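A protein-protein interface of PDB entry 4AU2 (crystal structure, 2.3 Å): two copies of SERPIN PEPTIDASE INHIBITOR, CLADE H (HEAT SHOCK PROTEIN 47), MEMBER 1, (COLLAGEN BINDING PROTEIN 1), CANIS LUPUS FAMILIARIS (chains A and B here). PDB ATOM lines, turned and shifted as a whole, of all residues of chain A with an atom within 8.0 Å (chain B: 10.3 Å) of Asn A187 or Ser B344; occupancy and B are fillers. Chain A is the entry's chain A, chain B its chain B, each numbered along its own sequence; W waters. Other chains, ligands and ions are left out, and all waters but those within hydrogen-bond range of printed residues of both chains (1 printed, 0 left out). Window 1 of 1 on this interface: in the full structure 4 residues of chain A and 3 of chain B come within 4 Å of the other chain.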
ATOM      1  N   VAL A 185       2.383   9.478 -12.660  1.00  0.00           N
ATOM      2  CA  VAL A 185       2.732  10.287 -13.824  1.00  0.00           C
ATOM      3  C   VAL A 185       1.448  10.775 -14.493  1.00  0.00           C
ATOM      4  O   VAL A 185       0.528   9.990 -14.729  1.00  0.00           O
ATOM      5  CB  VAL A 185       3.612   9.465 -14.815  1.00  0.00           C
ATOM      6  CG1 VAL A 185       4.088  10.292 -16.000  1.00  0.00           C
ATOM      7  CG2 VAL A 185       4.793   8.812 -14.113  1.00  0.00           C
ATOM      8  N   ASP A 186       1.384  12.078 -14.793  1.00  0.00           N
ATOM      9  CA  ASP A 186       0.216  12.680 -15.440  1.00  0.00           C
ATOM     10  C   ASP A 186       0.609  13.942 -16.169  1.00  0.00           C
ATOM     11  O   ASP A 186       1.768  14.345 -16.109  1.00  0.00           O
ATOM     12  CB  ASP A 186      -0.958  12.915 -14.443  1.00  0.00           C
ATOM     13  CG  ASP A 186      -0.645  13.743 -13.203  1.00  0.00           C
ATOM     14  OD1 ASP A 186       0.296  14.567 -13.255  1.00  0.00           O
ATOM     15  OD2 ASP A 186      -1.373  13.608 -12.204  1.00  0.00           O
ATOM     16  N   ASN A 187      -0.344  14.549 -16.862  1.00  0.00           N
ATOM     17  CA  ASN A 187      -0.162  15.754 -17.645  1.00  0.00           C
ATOM     18  C   ASN A 187      -0.478  16.999 -16.845  1.00  0.00           C
ATOM     19  O   ASN A 187      -1.531  17.099 -16.206  1.00  0.00           O
ATOM     20  CB  ASN A 187      -0.986  15.695 -18.934  1.00  0.00           C
ATOM     21  CG  ASN A 187      -0.583  14.552 -19.834  1.00  0.00           C
ATOM     22  OD1 ASN A 187       0.604  14.317 -20.113  1.00  0.00           O
ATOM     23  ND2 ASN A 187      -1.567  13.796 -20.292  1.00  0.00           N
ATOM     24  N   ARG A 188       0.463  17.930 -16.858  1.00  0.00           N
ATOM     25  CA  ARG A 188       0.364  19.193 -16.140  1.00  0.00           C
ATOM     26  C   ARG A 188       0.864  20.331 -17.040  1.00  0.00           C
ATOM     27  O   ARG A 188       1.503  20.086 -18.063  1.00  0.00           O
ATOM     28  CB  ARG A 188       1.209  19.132 -14.834  1.00  0.00           C
ATOM     29  CG  ARG A 188       0.882  17.975 -13.871  1.00  0.00           C
ATOM     30  CD  ARG A 188      -0.368  18.228 -13.067  1.00  0.00           C
ATOM     31  NE  ARG A 188      -0.811  17.040 -12.327  1.00  0.00           N
ATOM     32  CZ  ARG A 188      -0.929  16.984 -11.005  1.00  0.00           C
ATOM     33  NH1 ARG A 188      -0.613  18.035 -10.262  1.00  0.00           N
ATOM     34  NH2 ARG A 188      -1.360  15.872 -10.414  1.00  0.00           N
ATOM     35  N   GLY A 189       0.555  21.560 -16.653  1.00  0.00           N
ATOM     36  CA  GLY A 189       1.063  22.740 -17.337  1.00  0.00           C
ATOM     37  C   GLY A 189       2.321  23.250 -16.650  1.00  0.00           C
ATOM     38  O   GLY A 189       2.334  23.387 -15.421  1.00  0.00           O
ATOM     39  N   PHE A 190       3.402  23.497 -17.426  1.00  0.00           N
ATOM     40  CA  PHE A 190       4.634  24.094 -16.909  1.00  0.00           C
ATOM     41  C   PHE A 190       4.622  25.584 -17.290  1.00  0.00           C
ATOM     42  O   PHE A 190       4.516  25.933 -18.473  1.00  0.00           O
ATOM     43  CB  PHE A 190       5.897  23.397 -17.456  1.00  0.00           C
ATOM     44  CG  PHE A 190       7.216  23.867 -16.871  1.00  0.00           C
ATOM     45  CD1 PHE A 190       7.808  25.053 -17.298  1.00  0.00           C
ATOM     46  CD2 PHE A 190       7.895  23.096 -15.934  1.00  0.00           C
ATOM     47  CE1 PHE A 190       9.036  25.474 -16.770  1.00  0.00           C
ATOM     48  CE2 PHE A 190       9.122  23.525 -15.398  1.00  0.00           C
ATOM     49  CZ  PHE A 190       9.689  24.703 -15.830  1.00  0.00           C
ATOM     50  N   THR A 197       2.460  29.007 -20.871  1.00  0.00           N
ATOM     51  CA  THR A 197       2.376  27.669 -20.286  1.00  0.00           C
ATOM     52  C   THR A 197       2.569  26.601 -21.348  1.00  0.00           C
ATOM     53  O   THR A 197       1.930  26.646 -22.391  1.00  0.00           O
ATOM     54  CB  THR A 197       1.046  27.502 -19.508  1.00  0.00           C
ATOM     55  OG1 THR A 197       0.987  28.491 -18.478  1.00  0.00           O
ATOM     56  CG2 THR A 197       0.885  26.111 -18.883  1.00  0.00           C
ATOM     57  N   VAL A 198       3.418  25.622 -21.050  1.00  0.00           N
ATOM     58  CA  VAL A 198       3.709  24.484 -21.918  1.00  0.00           C
ATOM     59  C   VAL A 198       3.200  23.169 -21.278  1.00  0.00           C
ATOM     60  O   VAL A 198       3.357  22.954 -20.066  1.00  0.00           O
ATOM     61  CB  VAL A 198       5.220  24.454 -22.326  1.00  0.00           C
ATOM     62  CG1 VAL A 198       6.140  24.324 -21.123  1.00  0.00           C
ATOM     63  CG2 VAL A 198       5.512  23.369 -23.332  1.00  0.00           C
ATOM     64  N   GLY A 199       2.566  22.333 -22.099  1.00  0.00           N
ATOM     65  CA  GLY A 199       2.046  21.038 -21.685  1.00  0.00           C
ATOM     66  C   GLY A 199       3.169  20.057 -21.432  1.00  0.00           C
ATOM     67  O   GLY A 199       3.954  19.749 -22.334  1.00  0.00           O
ATOM     68  N   VAL A 200       3.294  19.602 -20.175  1.00  0.00           N
ATOM     69  CA  VAL A 200       4.345  18.677 -19.785  1.00  0.00           C
ATOM     70  C   VAL A 200       3.792  17.443 -19.076  1.00  0.00           C
ATOM     71  O   VAL A 200       2.656  17.420 -18.629  1.00  0.00           O
ATOM     72  CB  VAL A 200       5.518  19.359 -18.997  1.00  0.00           C
ATOM     73  CG1 VAL A 200       6.132  20.533 -19.738  1.00  0.00           C
ATOM     74  CG2 VAL A 200       5.156  19.716 -17.558  1.00  0.00           C
ATOM     75  N   THR A 201       4.616  16.421 -18.966  1.00  0.00           N
ATOM     76  CA  THR A 201       4.345  15.215 -18.202  1.00  0.00           C
ATOM     77  C   THR A 201       5.094  15.423 -16.870  1.00  0.00           C
ATOM     78  O   THR A 201       6.240  15.867 -16.876  1.00  0.00           O
ATOM     79  CB  THR A 201       4.802  14.004 -19.001  1.00  0.00           C
ATOM     80  OG1 THR A 201       3.891  13.814 -20.072  1.00  0.00           O
ATOM     81  CG2 THR A 201       4.838  12.755 -18.180  1.00  0.00           C
ATOM     82  N   MET A 202       4.419  15.185 -15.746  1.00  0.00           N
ATOM     83  CA  MET A 202       5.047  15.325 -14.429  1.00  0.00           C
ATOM     84  C   MET A 202       4.991  14.030 -13.644  1.00  0.00           C
ATOM     85  O   MET A 202       4.014  13.288 -13.750  1.00  0.00           O
ATOM     86  CB  MET A 202       4.416  16.466 -13.617  1.00  0.00           C
ATOM     87  CG  MET A 202       5.021  17.809 -13.925  1.00  0.00           C
ATOM     88  SD  MET A 202       4.386  19.106 -12.852  1.00  0.00           S
ATOM     89  CE  MET A 202       5.801  19.431 -11.879  1.00  0.00           C
ATOM     90  N   MET A 203       6.033  13.766 -12.843  1.00  0.00           N
ATOM     91  CA  MET A 203       6.120  12.592 -11.967  1.00  0.00           C
ATOM     92  C   MET A 203       6.030  13.116 -10.531  1.00  0.00           C
ATOM     93  O   MET A 203       6.504  14.224 -10.240  1.00  0.00           O
ATOM     94  CB  MET A 203       7.390  11.751 -12.221  1.00  0.00           C
ATOM     95  CG  MET A 203       8.664  12.552 -12.203  1.00  0.00           C
ATOM     96  SD  MET A 203      10.147  11.577 -12.533  1.00  0.00           S
ATOM     97  CE  MET A 203      11.409  12.794 -12.189  1.00  0.00           C
ATOM     98  N   HIS A 204       5.365  12.355  -9.657  1.00  0.00           N
ATOM     99  CA  HIS A 204       5.084  12.794  -8.295  1.00  0.00           C
ATOM    100  C   HIS A 204       5.466  11.762  -7.273  1.00  0.00           C
ATOM    101  O   HIS A 204       5.187  10.577  -7.461  1.00  0.00           O
ATOM    102  CB  HIS A 204       3.569  13.106  -8.141  1.00  0.00           C
ATOM    103  CG  HIS A 204       2.980  13.879  -9.287  1.00  0.00           C
ATOM    104  ND1 HIS A 204       2.854  15.264  -9.249  1.00  0.00           N
ATOM    105  CD2 HIS A 204       2.518  13.438 -10.480  1.00  0.00           C
ATOM    106  CE1 HIS A 204       2.314  15.611 -10.405  1.00  0.00           C
ATOM    107  NE2 HIS A 204       2.108  14.551 -11.184  1.00  0.00           N
ATOM    108  N   TYR A 349       6.500  21.736  -5.972  1.00  0.00           N
ATOM    109  CA  TYR A 349       5.796  21.644  -7.253  1.00  0.00           C
ATOM    110  C   TYR A 349       6.568  22.413  -8.327  1.00  0.00           C
ATOM    111  O   TYR A 349       6.394  23.623  -8.492  1.00  0.00           O
ATOM    112  CB  TYR A 349       4.351  22.168  -7.044  1.00  0.00           C
ATOM    113  CG  TYR A 349       3.341  21.721  -8.075  1.00  0.00           C
ATOM    114  CD1 TYR A 349       2.676  20.507  -7.945  1.00  0.00           C
ATOM    115  CD2 TYR A 349       3.008  22.536  -9.151  1.00  0.00           C
ATOM    116  CE1 TYR A 349       1.718  20.105  -8.875  1.00  0.00           C
ATOM    117  CE2 TYR A 349       2.050  22.148 -10.082  1.00  0.00           C
ATOM    118  CZ  TYR A 349       1.418  20.926  -9.949  1.00  0.00           C
ATOM    119  OH  TYR A 349       0.488  20.556 -10.886  1.00  0.00           O
ATOM    120  N   MET A 380       0.185  25.964 -24.348  1.00  0.00           N
ATOM    121  CA  MET A 380      -1.239  25.858 -23.984  1.00  0.00           C
ATOM    122  C   MET A 380      -1.809  27.162 -23.428  1.00  0.00           C
ATOM    123  O   MET A 380      -2.154  28.054 -24.199  1.00  0.00           O
ATOM    124  CB  MET A 380      -1.527  24.657 -23.043  1.00  0.00           C
ATOM    125  CG  MET A 380      -0.620  24.574 -21.826  1.00  0.00           C
ATOM    126  SD  MET A 380      -0.992  23.204 -20.705  1.00  0.00           S
ATOM    127  CE  MET A 380      -2.182  23.992 -19.643  1.00  0.00           C
ATOM    128  N   THR B 206     -12.059  16.045 -11.671  1.00  0.00           N
ATOM    129  CA  THR B 206     -11.481  16.193 -13.001  1.00  0.00           C
ATOM    130  C   THR B 206     -12.039  15.073 -13.889  1.00  0.00           C
ATOM    131  O   THR B 206     -12.032  13.906 -13.486  1.00  0.00           O
ATOM    132  CB  THR B 206      -9.943  16.214 -12.959  1.00  0.00           C
ATOM    133  OG1 THR B 206      -9.542  17.318 -12.157  1.00  0.00           O
ATOM    134  CG2 THR B 206      -9.333  16.391 -14.334  1.00  0.00           C
ATOM    135  N   GLY B 207     -12.506  15.437 -15.078  1.00  0.00           N
ATOM    136  CA  GLY B 207     -13.053  14.479 -16.026  1.00  0.00           C
ATOM    137  C   GLY B 207     -13.236  15.115 -17.376  1.00  0.00           C
ATOM    138  O   GLY B 207     -12.952  16.305 -17.545  1.00  0.00           O
ATOM    139  N   LEU B 208     -13.739  14.322 -18.338  1.00  0.00           N
ATOM    140  CA  LEU B 208     -13.986  14.736 -19.716  1.00  0.00           C
ATOM    141  C   LEU B 208     -15.370  15.364 -19.783  1.00  0.00           C
ATOM    142  O   LEU B 208     -16.377  14.693 -19.523  1.00  0.00           O
ATOM    143  CB  LEU B 208     -13.858  13.525 -20.660  1.00  0.00           C
ATOM    144  CG  LEU B 208     -13.126  13.742 -21.982  1.00  0.00           C
ATOM    145  CD1 LEU B 208     -11.661  14.162 -21.770  1.00  0.00           C
ATOM    146  CD2 LEU B 208     -13.177  12.478 -22.828  1.00  0.00           C
ATOM    147  N   TYR B 211     -17.075  21.483 -23.046  1.00  0.00           N
ATOM    148  CA  TYR B 211     -16.597  22.752 -22.548  1.00  0.00           C
ATOM    149  C   TYR B 211     -16.306  23.721 -23.677  1.00  0.00           C
ATOM    150  O   TYR B 211     -15.944  23.323 -24.790  1.00  0.00           O
ATOM    151  CB  TYR B 211     -15.316  22.469 -21.749  1.00  0.00           C
ATOM    152  CG  TYR B 211     -14.540  23.666 -21.244  1.00  0.00           C
ATOM    153  CD1 TYR B 211     -14.831  24.238 -20.007  1.00  0.00           C
ATOM    154  CD2 TYR B 211     -13.451  24.163 -21.953  1.00  0.00           C
ATOM    155  CE1 TYR B 211     -14.094  25.315 -19.518  1.00  0.00           C
ATOM    156  CE2 TYR B 211     -12.712  25.240 -21.477  1.00  0.00           C
ATOM    157  CZ  TYR B 211     -13.033  25.809 -20.255  1.00  0.00           C
ATOM    158  OH  TYR B 211     -12.309  26.875 -19.784  1.00  0.00           O
ATOM    159  N   LYS B 265     -15.596  18.097 -25.979  1.00  0.00           N
ATOM    160  CA  LYS B 265     -15.183  17.295 -24.831  1.00  0.00           C
ATOM    161  C   LYS B 265     -13.716  17.517 -24.522  1.00  0.00           C
ATOM    162  O   LYS B 265     -12.868  17.266 -25.372  1.00  0.00           O
ATOM    163  CB  LYS B 265     -15.519  15.811 -25.023  1.00  0.00           C
ATOM    164  CG  LYS B 265     -16.958  15.495 -24.646  1.00  0.00           C
ATOM    165  CD  LYS B 265     -17.129  14.080 -24.125  1.00  0.00           C
ATOM    166  CE  LYS B 265     -18.556  13.790 -23.729  1.00  0.00           C
ATOM    167  NZ  LYS B 265     -19.440  13.628 -24.912  1.00  0.00           N
ATOM    168  N   LYS B 266     -13.434  18.055 -23.312  1.00  0.00           N
ATOM    169  CA  LYS B 266     -12.085  18.399 -22.833  1.00  0.00           C
ATOM    170  C   LYS B 266     -11.894  18.009 -21.372  1.00  0.00           C
ATOM    171  O   LYS B 266     -12.879  17.845 -20.645  1.00  0.00           O
ATOM    172  CB  LYS B 266     -11.824  19.917 -22.997  1.00  0.00           C
ATOM    173  CG  LYS B 266     -11.462  20.340 -24.418  1.00  0.00           C
ATOM    174  CD  LYS B 266     -11.315  21.857 -24.522  1.00  0.00           C
ATOM    175  CE  LYS B 266     -11.176  22.368 -25.937  1.00  0.00           C
ATOM    176  NZ  LYS B 266      -9.980  21.827 -26.655  1.00  0.00           N
ATOM    177  N   ALA B 267     -10.624  17.882 -20.932  1.00  0.00           N
ATOM    178  CA  ALA B 267     -10.319  17.597 -19.530  1.00  0.00           C
ATOM    179  C   ALA B 267     -10.573  18.885 -18.744  1.00  0.00           C
ATOM    180  O   ALA B 267      -9.988  19.934 -19.032  1.00  0.00           O
ATOM    181  CB  ALA B 267      -8.887  17.150 -19.378  1.00  0.00           C
ATOM    182  N   VAL B 268     -11.547  18.833 -17.845  1.00  0.00           N
ATOM    183  CA  VAL B 268     -11.935  19.985 -17.047  1.00  0.00           C
ATOM    184  C   VAL B 268     -11.905  19.600 -15.573  1.00  0.00           C
ATOM    185  O   VAL B 268     -12.481  18.566 -15.195  1.00  0.00           O
ATOM    186  CB  VAL B 268     -13.319  20.585 -17.455  1.00  0.00           C
ATOM    187  CG1 VAL B 268     -13.592  21.890 -16.710  1.00  0.00           C
ATOM    188  CG2 VAL B 268     -13.431  20.806 -18.964  1.00  0.00           C
ATOM    189  N   ALA B 269     -11.210  20.423 -14.752  1.00  0.00           N
ATOM    190  CA  ALA B 269     -11.165  20.255 -13.290  1.00  0.00           C
ATOM    191  C   ALA B 269     -12.252  21.200 -12.771  1.00  0.00           C
ATOM    192  O   ALA B 269     -12.087  22.429 -12.802  1.00  0.00           O
ATOM    193  CB  ALA B 269      -9.795  20.640 -12.733  1.00  0.00           C
ATOM    194  N   GLU B 341      -3.943   8.873 -21.013  1.00  0.00           N
ATOM    195  CA  GLU B 341      -4.971   9.419 -20.133  1.00  0.00           C
ATOM    196  C   GLU B 341      -5.310  10.883 -20.490  1.00  0.00           C
ATOM    197  O   GLU B 341      -4.862  11.367 -21.535  1.00  0.00           O
ATOM    198  CB  GLU B 341      -4.559   9.259 -18.657  1.00  0.00           C
ATOM    199  N   LEU B 342      -6.131  11.568 -19.642  1.00  0.00           N
ATOM    200  CA  LEU B 342      -6.582  12.961 -19.803  1.00  0.00           C
ATOM    201  C   LEU B 342      -5.421  13.961 -19.895  1.00  0.00           C
ATOM    202  O   LEU B 342      -4.381  13.757 -19.261  1.00  0.00           O
ATOM    203  CB  LEU B 342      -7.476  13.369 -18.637  1.00  0.00           C
ATOM    204  CG  LEU B 342      -8.809  12.645 -18.486  1.00  0.00           C
ATOM    205  CD1 LEU B 342      -8.871  11.900 -17.155  1.00  0.00           C
ATOM    206  CD2 LEU B 342      -9.963  13.624 -18.553  1.00  0.00           C
ATOM    207  N   ARG B 343      -5.611  15.049 -20.672  1.00  0.00           N
ATOM    208  CA  ARG B 343      -4.629  16.129 -20.836  1.00  0.00           C
ATOM    209  C   ARG B 343      -4.713  17.083 -19.633  1.00  0.00           C
ATOM    210  O   ARG B 343      -5.686  17.021 -18.884  1.00  0.00           O
ATOM    211  CB  ARG B 343      -4.877  16.901 -22.148  1.00  0.00           C
ATOM    212  CG  ARG B 343      -4.660  16.072 -23.408  1.00  0.00           C
ATOM    213  CD  ARG B 343      -4.480  16.931 -24.643  1.00  0.00           C
ATOM    214  NE  ARG B 343      -3.311  16.502 -25.420  1.00  0.00           N
ATOM    215  CZ  ARG B 343      -2.963  17.000 -26.603  1.00  0.00           C
ATOM    216  NH1 ARG B 343      -3.695  17.950 -27.174  1.00  0.00           N
ATOM    217  NH2 ARG B 343      -1.882  16.550 -27.226  1.00  0.00           N
ATOM    218  N   SER B 344      -3.682  17.940 -19.441  1.00  0.00           N
ATOM    219  CA  SER B 344      -3.549  18.976 -18.411  1.00  0.00           C
ATOM    220  C   SER B 344      -4.915  19.675 -18.355  1.00  0.00           C
ATOM    221  O   SER B 344      -5.304  20.232 -19.377  1.00  0.00           O
ATOM    222  CB  SER B 344      -2.448  19.940 -18.845  1.00  0.00           C
ATOM    223  OG  SER B 344      -2.367  21.079 -18.006  1.00  0.00           O
ATOM    224  N   PRO B 345      -5.733  19.537 -17.287  1.00  0.00           N
ATOM    225  CA  PRO B 345      -7.098  20.075 -17.361  1.00  0.00           C
ATOM    226  C   PRO B 345      -7.262  21.575 -17.295  1.00  0.00           C
ATOM    227  O   PRO B 345      -6.408  22.274 -16.759  1.00  0.00           O
ATOM    228  CB  PRO B 345      -7.824  19.380 -16.201  1.00  0.00           C
ATOM    229  CG  PRO B 345      -6.770  19.150 -15.210  1.00  0.00           C
ATOM    230  CD  PRO B 345      -5.506  18.858 -15.993  1.00  0.00           C
ATOM    231  N   LYS B 346      -8.370  22.059 -17.865  1.00  0.00           N
ATOM    232  CA  LYS B 346      -8.753  23.466 -17.813  1.00  0.00           C
ATOM    233  C   LYS B 346      -9.474  23.606 -16.492  1.00  0.00           C
ATOM    234  O   LYS B 346     -10.207  22.684 -16.101  1.00  0.00           O
ATOM    235  CB  LYS B 346      -9.734  23.829 -18.951  1.00  0.00           C
ATOM    236  CG  LYS B 346      -9.276  23.510 -20.379  1.00  0.00           C
ATOM    237  CD  LYS B 346      -8.260  24.488 -20.923  1.00  0.00           C
ATOM    238  CE  LYS B 346      -8.065  24.334 -22.414  1.00  0.00           C
ATOM    239  NZ  LYS B 346      -9.118  25.072 -23.182  1.00  0.00           N
ATOM    240  N   LEU B 347      -9.266  24.722 -15.783  1.00  0.00           N
ATOM    241  CA  LEU B 347      -9.978  24.899 -14.508  1.00  0.00           C
ATOM    242  C   LEU B 347     -11.336  25.559 -14.715  1.00  0.00           C
ATOM    243  O   LEU B 347     -11.436  26.512 -15.491  1.00  0.00           O
ATOM    244  CB  LEU B 347      -9.159  25.715 -13.477  1.00  0.00           C
ATOM    245  CG  LEU B 347      -7.762  25.213 -13.107  1.00  0.00           C
ATOM    246  CD1 LEU B 347      -7.063  26.210 -12.204  1.00  0.00           C
ATOM    247  CD2 LEU B 347      -7.806  23.847 -12.428  1.00  0.00           C
ATOM    248  N   PHE B 348     -12.371  25.033 -14.039  1.00  0.00           N
ATOM    249  CA  PHE B 348     -13.716  25.609 -13.968  1.00  0.00           C
ATOM    250  C   PHE B 348     -13.926  25.753 -12.468  1.00  0.00           C
ATOM    251  O   PHE B 348     -14.545  24.910 -11.824  1.00  0.00           O
ATOM    252  CB  PHE B 348     -14.801  24.734 -14.632  1.00  0.00           C
ATOM    253  CG  PHE B 348     -16.081  25.517 -14.877  1.00  0.00           C
ATOM    254  CD1 PHE B 348     -17.007  25.709 -13.856  1.00  0.00           C
ATOM    255  CD2 PHE B 348     -16.333  26.103 -16.116  1.00  0.00           C
ATOM    256  CE1 PHE B 348     -18.150  26.471 -14.069  1.00  0.00           C
ATOM    257  CE2 PHE B 348     -17.488  26.854 -16.329  1.00  0.00           C
ATOM    258  CZ  PHE B 348     -18.386  27.033 -15.305  1.00  0.00           C
HETATM  259  O   HOH W   1      -1.654  21.650 -14.656  1.00  0.00           O
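The backbone NH of Val A200 lies within hydrogen-bond range of the backbone carbonyl oxygen of Arg A188 (2.8 Å).
The side-chain hydroxyl (OH) of Tyr A349 sits at hydrogen-bond distance from the guanidinium group (NH1) of Arg A188.
The side-chain amide oxygen (OD1) of Asn A187 is in hydrogen-bond range of the side-chain hydroxyl (OG1) of Thr A201.
The side-chain carboxylate (OD1) of Asp A186 lies within salt-bridge range of the guanidinium group (NE) of Arg A188 (2.9 Å).
The backbone carbonyl oxygen (O) of Thr A197 sits at hydrogen-bond distance from the backbone NH (N) of Met A380 (2.7 Å).
Water W1 lies within hydrogen-bond range of the backbone NH (N) of Gly A189 (3.0 Å) and the side-chain hydroxyl (OG) of Ser B344 (3.5 Å).
Of the 17 printed residues of chain B, 3 touch a printed residue of chain A.
Printed residues of chain B that touch a printed residue of chain A: Leu B342, Arg B343 and Ser B344.
Of the 16 printed residues of chain A, 4 touch a printed residue of chain B.
Hydrophobic or aromatic side chains of chain A that line the printed part of chain B: Met A380.
Among the printed residues, no Asp or Glu carboxylate lies within 4 Å of a Lys or Arg side-chain nitrogen of the other chain.
Among the printed residues, merely in contact across the chains: Asn A187 with Arg B343 (3.9 Å), Asn A187 with Ser B344 (3.5 Å) and Arg A188 with Ser B344 (3.5 Å).
SD of Met A380 sits close to OG of Ser B344, at 3.7 Å.
The backbone carbonyl oxygen of Leu B342 lies within hydrogen-bond range of the side-chain amide nitrogen of Asn A187 (3.0 Å).
N of Gly A189 lies within hydrogen-bond range of OG of Ser B344, 3.3 Å away.
Of chain B, only Leu B342, Arg B343 and Ser B344 come within 4 Å of Asn A187.
Of chain B, only Ser B344 (3.3 Å) comes within 4 Å of Gly A189.
Printed residues of chain B within 4 Å of Met A380: Ser B344 (3.3 Å).
Lys B266 touches none of the printed residues of chain A.
Printed residues of chain A within 4 Å of Leu B342: Asn A187.
Of the printed residues of chain A, Arg B343 touches Asn A187 (3.9 Å).
Of the printed residues of chain A, Ser B344 touches Asn A187, Arg A188, Gly A189 and Met A380.
No residue of chain A comes within 4 Å of Pro B345.
Leu B347 touches none of the printed residues of chain A.
The nearest residue of chain B that does not touch Asn A187 is Glu B341 (4.3 Å).
The nearest residue of chain A that does not touch Ser B344 is Gly A199 (5.4 Å).
The nearest printed residue of chain A that does not touch Leu B342 is Asp A186 (5.9 Å).
No position is printed for both chains.
Of the 6 pairs that touch across the chains among the printed residues, none has its exchanged pair printed and touching as well.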
